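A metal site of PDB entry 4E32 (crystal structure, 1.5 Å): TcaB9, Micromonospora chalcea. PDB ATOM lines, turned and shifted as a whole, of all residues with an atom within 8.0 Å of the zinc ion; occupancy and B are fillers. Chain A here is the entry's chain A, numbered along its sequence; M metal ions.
The backbone NH of Gly 20 lies close to the side-chain sulfur of Cys 18, 3.3 Å away. The backbone NH (N) of Ser 58 sits close to the side-chain sulfur (SG) of Cys 56 (3.2 Å). The side-chain sulfur of Cys 15 lies close to the backbone NH of Val 17 (3.3 Å). The backbone NH (N) of Cys 56 sits at hydrogen-bond distance from the backbone carbonyl oxygen (O) of Met 61 (2.9 Å). The side-chain sulfur (SG) of Cys 59 sits close to the backbone NH (N) of Met 61, at 3.5 Å. The side-chain amide nitrogen (NE2) of Gln 63 lies close to the side-chain sulfur (SG) of Cys 15 (3.4 Å). The backbone NH (N) of Cys 15 sits at hydrogen-bond distance from the backbone carbonyl oxygen (O) of Gly 20 (2.8 Å).
Within 4 Å of the zinc ion: Cys 15, Cys 18, Cys 56 and Cys 59. The nearest printed residue that does not touch the zinc ion is Val 17 (4.4 Å).
The zinc ion is bound by the side-chain sulfur (SG) of Cys 59 (2.3 Å), the side-chain sulfur (SG) of Cys 15 (2.3 Å), the side-chain sulfur (SG) of Cys 18 (2.3 Å) and the side-chain sulfur (SG) of Cys 56 (2.4 Å). The zinc ion has four donor atoms within binding distance.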
ATOM      1  N   ALA A  14      -7.669  28.902 -27.869  1.00  0.00           N
ATOM      2  CA  ALA A  14      -7.241  27.906 -26.876  1.00  0.00           C
ATOM      3  C   ALA A  14      -5.998  28.415 -26.119  1.00  0.00           C
ATOM      4  O   ALA A  14      -5.045  28.905 -26.737  1.00  0.00           O
ATOM      5  CB  ALA A  14      -6.908  26.570 -27.549  1.00  0.00           C
ATOM      6  N   CYS A  15      -6.024  28.293 -24.802  1.00  0.00           N
ATOM      7  CA  CYS A  15      -4.854  28.528 -23.946  1.00  0.00           C
ATOM      8  C   CYS A  15      -3.642  27.743 -24.442  1.00  0.00           C
ATOM      9  O   CYS A  15      -3.746  26.537 -24.679  1.00  0.00           O
ATOM     10  CB  CYS A  15      -5.194  28.080 -22.525  1.00  0.00           C
ATOM     11  SG  CYS A  15      -3.811  28.335 -21.391  1.00  0.00           S
ATOM     12  N   ARG A  16      -2.518  28.438 -24.600  1.00  0.00           N
ATOM     13  CA  ARG A  16      -1.280  27.786 -25.038  1.00  0.00           C
ATOM     14  C   ARG A  16      -0.613  26.970 -23.919  1.00  0.00           C
ATOM     15  O   ARG A  16       0.312  26.214 -24.201  1.00  0.00           O
ATOM     16  CB  ARG A  16      -0.337  28.853 -25.631  1.00  0.00           C
ATOM     17  CG  ARG A  16      -0.710  29.268 -27.052  1.00  0.00           C
ATOM     18  CD  ARG A  16      -0.497  28.027 -27.932  1.00  0.00           C
ATOM     19  NE  ARG A  16       0.325  28.434 -29.054  1.00  0.00           N
ATOM     20  CZ  ARG A  16       1.404  27.818 -29.511  1.00  0.00           C
ATOM     21  NH1 ARG A  16       1.964  28.392 -30.569  1.00  0.00           N
ATOM     22  NH2 ARG A  16       1.876  26.672 -29.041  1.00  0.00           N
ATOM     23  N   VAL A  17      -1.086  27.117 -22.685  1.00  0.00           N
ATOM     24  CA  VAL A  17      -0.569  26.315 -21.579  1.00  0.00           C
ATOM     25  C   VAL A  17      -1.340  24.996 -21.471  1.00  0.00           C
ATOM     26  O   VAL A  17      -0.688  23.932 -21.429  1.00  0.00           O
ATOM     27  CB  VAL A  17      -0.540  27.058 -20.210  1.00  0.00           C
ATOM     28  CG1 VAL A  17      -0.045  26.132 -19.093  1.00  0.00           C
ATOM     29  CG2 VAL A  17       0.402  28.260 -20.287  1.00  0.00           C
ATOM     30  N   CYS A  18      -2.670  25.054 -21.455  1.00  0.00           N
ATOM     31  CA  CYS A  18      -3.489  23.909 -21.058  1.00  0.00           C
ATOM     32  C   CYS A  18      -4.621  23.541 -22.022  1.00  0.00           C
ATOM     33  O   CYS A  18      -5.296  22.516 -21.849  1.00  0.00           O
ATOM     34  CB  CYS A  18      -4.081  24.116 -19.652  1.00  0.00           C
ATOM     35  SG  CYS A  18      -5.497  25.224 -19.635  1.00  0.00           S
ATOM     36  N   GLY A  19      -4.853  24.381 -23.014  1.00  0.00           N
ATOM     37  CA  GLY A  19      -5.922  24.150 -23.991  1.00  0.00           C
ATOM     38  C   GLY A  19      -7.305  24.626 -23.552  1.00  0.00           C
ATOM     39  O   GLY A  19      -8.247  24.509 -24.339  1.00  0.00           O
ATOM     40  N   GLY A  20      -7.428  25.217 -22.364  1.00  0.00           N
ATOM     41  CA  GLY A  20      -8.674  25.809 -21.909  1.00  0.00           C
ATOM     42  C   GLY A  20      -9.128  26.960 -22.794  1.00  0.00           C
ATOM     43  O   GLY A  20      -8.427  27.391 -23.707  1.00  0.00           O
ATOM     44  N   GLY A  21     -10.307  27.512 -22.498  1.00  0.00           N
ATOM     45  CA  GLY A  21     -10.819  28.674 -23.227  1.00  0.00           C
ATOM     46  C   GLY A  21     -10.333  29.994 -22.661  1.00  0.00           C
ATOM     47  O   GLY A  21     -10.335  30.210 -21.438  1.00  0.00           O
ATOM     48  N   VAL A  22      -9.907  30.874 -23.554  1.00  0.00           N
ATOM     49  CA  VAL A  22      -9.375  32.175 -23.142  1.00  0.00           C
ATOM     50  C   VAL A  22     -10.471  33.207 -23.359  1.00  0.00           C
ATOM     51  O   VAL A  22     -10.940  33.355 -24.501  1.00  0.00           O
ATOM     52  CB  VAL A  22      -8.107  32.553 -23.943  1.00  0.00           C
ATOM     53  CG1 VAL A  22      -7.605  33.951 -23.633  1.00  0.00           C
ATOM     54  CG2 VAL A  22      -6.968  31.513 -23.687  1.00  0.00           C
ATOM     55  N   ARG A  55      -7.837  35.574 -20.600  1.00  0.00           N
ATOM     56  CA  ARG A  55      -7.425  34.828 -19.430  1.00  0.00           C
ATOM     57  C   ARG A  55      -8.012  33.449 -19.632  1.00  0.00           C
ATOM     58  O   ARG A  55      -9.202  33.282 -19.914  1.00  0.00           O
ATOM     59  CB  ARG A  55      -7.944  35.411 -18.099  1.00  0.00           C
ATOM     60  CG  ARG A  55      -7.370  34.618 -16.926  1.00  0.00           C
ATOM     61  CD  ARG A  55      -8.202  34.644 -15.647  1.00  0.00           C
ATOM     62  NE  ARG A  55      -9.380  33.818 -15.856  1.00  0.00           N
ATOM     63  CZ  ARG A  55     -10.363  33.707 -14.969  1.00  0.00           C
ATOM     64  NH1 ARG A  55     -11.387  32.926 -15.294  1.00  0.00           N
ATOM     65  NH2 ARG A  55     -10.305  34.332 -13.797  1.00  0.00           N
ATOM     66  N   CYS A  56      -7.146  32.461 -19.429  1.00  0.00           N
ATOM     67  CA  CYS A  56      -7.696  31.127 -19.607  1.00  0.00           C
ATOM     68  C   CYS A  56      -8.625  30.781 -18.450  1.00  0.00           C
ATOM     69  O   CYS A  56      -8.289  31.036 -17.291  1.00  0.00           O
ATOM     70  CB  CYS A  56      -6.527  30.134 -19.506  1.00  0.00           C
ATOM     71  SG  CYS A  56      -7.068  28.400 -19.526  1.00  0.00           S
ATOM     72  N   ASP A  57      -9.723  30.117 -18.775  1.00  0.00           N
ATOM     73  CA  ASP A  57     -10.719  29.723 -17.783  1.00  0.00           C
ATOM     74  C   ASP A  57     -10.248  28.596 -16.874  1.00  0.00           C
ATOM     75  O   ASP A  57     -10.839  28.324 -15.819  1.00  0.00           O
ATOM     76  CB  ASP A  57     -11.979  29.244 -18.502  1.00  0.00           C
ATOM     77  CG  ASP A  57     -12.732  30.381 -19.133  1.00  0.00           C
ATOM     78  OD1 ASP A  57     -12.480  31.496 -18.637  1.00  0.00           O
ATOM     79  OD2 ASP A  57     -13.511  30.129 -20.078  1.00  0.00           O
ATOM     80  N   SER A  58      -9.221  27.871 -17.273  1.00  0.00           N
ATOM     81  CA  SER A  58      -8.828  26.687 -16.527  1.00  0.00           C
ATOM     82  C   SER A  58      -7.558  26.836 -15.726  1.00  0.00           C
ATOM     83  O   SER A  58      -7.490  26.322 -14.604  1.00  0.00           O
ATOM     84  CB  SER A  58      -8.649  25.459 -17.435  1.00  0.00           C
ATOM     85  OG  SER A  58      -9.886  25.256 -18.088  1.00  0.00           O
ATOM     86  N   CYS A  59      -6.538  27.479 -16.280  1.00  0.00           N
ATOM     87  CA  CYS A  59      -5.295  27.618 -15.540  1.00  0.00           C
ATOM     88  C   CYS A  59      -4.995  29.058 -15.111  1.00  0.00           C
ATOM     89  O   CYS A  59      -4.016  29.267 -14.411  1.00  0.00           O
ATOM     90  CB  CYS A  59      -4.119  27.050 -16.341  1.00  0.00           C
ATOM     91  SG  CYS A  59      -3.696  28.169 -17.713  1.00  0.00           S
ATOM     92  N   GLU A  60      -5.862  29.998 -15.493  1.00  0.00           N
ATOM     93  CA  GLU A  60      -5.734  31.418 -15.170  1.00  0.00           C
ATOM     94  C   GLU A  60      -4.599  32.169 -15.870  1.00  0.00           C
ATOM     95  O   GLU A  60      -4.343  33.328 -15.506  1.00  0.00           O
ATOM     96  CB  GLU A  60      -5.808  31.738 -13.660  1.00  0.00           C
ATOM     97  CG  GLU A  60      -7.089  31.106 -13.088  1.00  0.00           C
ATOM     98  CD  GLU A  60      -7.156  31.361 -11.580  1.00  0.00           C
ATOM     99  OE1 GLU A  60      -7.395  32.525 -11.214  1.00  0.00           O
ATOM    100  OE2 GLU A  60      -6.952  30.441 -10.749  1.00  0.00           O
ATOM    101  N   MET A  61      -3.957  31.513 -16.835  1.00  0.00           N
ATOM    102  CA  MET A  61      -2.894  32.170 -17.605  1.00  0.00           C
ATOM    103  C   MET A  61      -3.491  33.339 -18.405  1.00  0.00           C
ATOM    104  O   MET A  61      -4.334  33.149 -19.282  1.00  0.00           O
ATOM    105  CB  MET A  61      -2.177  31.219 -18.576  1.00  0.00           C
ATOM    106  CG  MET A  61      -1.013  31.906 -19.287  1.00  0.00           C
ATOM    107  SD  MET A  61       0.282  32.489 -18.173  1.00  0.00           S
ATOM    108  CE  MET A  61       1.092  30.970 -17.664  1.00  0.00           C
ATOM    109  N   VAL A  62      -2.981  34.551 -18.183  1.00  0.00           N
ATOM    110  CA  VAL A  62      -3.340  35.736 -18.987  1.00  0.00           C
ATOM    111  C   VAL A  62      -2.396  35.796 -20.195  1.00  0.00           C
ATOM    112  O   VAL A  62      -1.183  35.744 -20.024  1.00  0.00           O
ATOM    113  CB  VAL A  62      -3.120  37.015 -18.140  1.00  0.00           C
ATOM    114  CG1 VAL A  62      -3.286  38.248 -19.044  1.00  0.00           C
ATOM    115  CG2 VAL A  62      -4.178  37.012 -16.996  1.00  0.00           C
ATOM    116  N   GLN A  63      -2.941  35.935 -21.408  1.00  0.00           N
ATOM    117  CA  GLN A  63      -2.187  35.804 -22.650  1.00  0.00           C
ATOM    118  C   GLN A  63      -2.895  36.525 -23.796  1.00  0.00           C
ATOM    119  O   GLN A  63      -4.088  36.795 -23.734  1.00  0.00           O
ATOM    120  CB  GLN A  63      -2.041  34.334 -23.097  1.00  0.00           C
ATOM    121  CG  GLN A  63      -3.413  33.646 -23.281  1.00  0.00           C
ATOM    122  CD  GLN A  63      -3.309  32.147 -23.049  1.00  0.00           C
ATOM    123  OE1 GLN A  63      -2.926  31.414 -23.981  1.00  0.00           O
ATOM    124  NE2 GLN A  63      -3.590  31.697 -21.828  1.00  0.00           N
ATOM    125  N   PHE A 229       2.553  36.394 -22.789  1.00  0.00           N
ATOM    126  CA  PHE A 229       2.047  36.011 -21.473  1.00  0.00           C
ATOM    127  C   PHE A 229       2.216  37.133 -20.458  1.00  0.00           C
ATOM    128  O   PHE A 229       3.252  37.806 -20.428  1.00  0.00           O
ATOM    129  CB  PHE A 229       2.764  34.755 -20.937  1.00  0.00           C
ATOM    130  CG  PHE A 229       2.418  33.512 -21.722  1.00  0.00           C
ATOM    131  CD1 PHE A 229       1.140  32.965 -21.740  1.00  0.00           C
ATOM    132  CD2 PHE A 229       3.429  32.872 -22.414  1.00  0.00           C
ATOM    133  CE1 PHE A 229       0.872  31.820 -22.481  1.00  0.00           C
ATOM    134  CE2 PHE A 229       3.160  31.733 -23.147  1.00  0.00           C
ATOM    135  CZ  PHE A 229       1.902  31.166 -23.171  1.00  0.00           C
ATOM    136  N   SER A 235      -0.699  31.470 -12.179  1.00  0.00           N
ATOM    137  CA  SER A 235      -0.624  30.793 -13.488  1.00  0.00           C
ATOM    138  C   SER A 235       0.677  30.009 -13.666  1.00  0.00           C
ATOM    139  O   SER A 235       0.690  28.921 -14.231  1.00  0.00           O
ATOM    140  CB  SER A 235      -0.935  31.837 -14.569  1.00  0.00           C
ATOM    141  OG  SER A 235       0.138  32.767 -14.709  1.00  0.00           O
ATOM    142  N   MET A 239       1.108  26.219 -14.560  1.00  0.00           N
ATOM    143  CA  MET A 239       1.899  25.837 -15.723  1.00  0.00           C
ATOM    144  C   MET A 239       3.032  24.869 -15.383  1.00  0.00           C
ATOM    145  O   MET A 239       3.250  23.885 -16.086  1.00  0.00           O
ATOM    146  CB  MET A 239       2.480  27.124 -16.334  1.00  0.00           C
ATOM    147  CG  MET A 239       3.414  26.849 -17.510  1.00  0.00           C
ATOM    148  SD  MET A 239       4.088  28.347 -18.322  1.00  0.00           S
ATOM    149  CE  MET A 239       5.229  29.002 -17.102  1.00  0.00           C
ATOM    150  N   ARG A 242       1.572  21.370 -14.504  1.00  0.00           N
ATOM    151  CA  ARG A 242       1.002  20.635 -15.631  1.00  0.00           C
ATOM    152  C   ARG A 242       2.089  20.080 -16.534  1.00  0.00           C
ATOM    153  O   ARG A 242       1.848  19.192 -17.359  1.00  0.00           O
ATOM    154  CB  ARG A 242       0.065  21.510 -16.469  1.00  0.00           C
ATOM    155  CG  ARG A 242      -1.305  21.747 -15.851  1.00  0.00           C
ATOM    156  CD  ARG A 242      -1.885  23.017 -16.483  1.00  0.00           C
ATOM    157  NE  ARG A 242      -3.315  23.113 -16.251  1.00  0.00           N
ATOM    158  CZ  ARG A 242      -3.941  23.710 -15.240  1.00  0.00           C
ATOM    159  NH1 ARG A 242      -3.299  24.361 -14.264  1.00  0.00           N
ATOM    160  NH2 ARG A 242      -5.260  23.659 -15.255  1.00  0.00           N
HETATM  161 ZN    ZN M   1      -4.873  27.457 -19.527  1.00  0.00          ZN
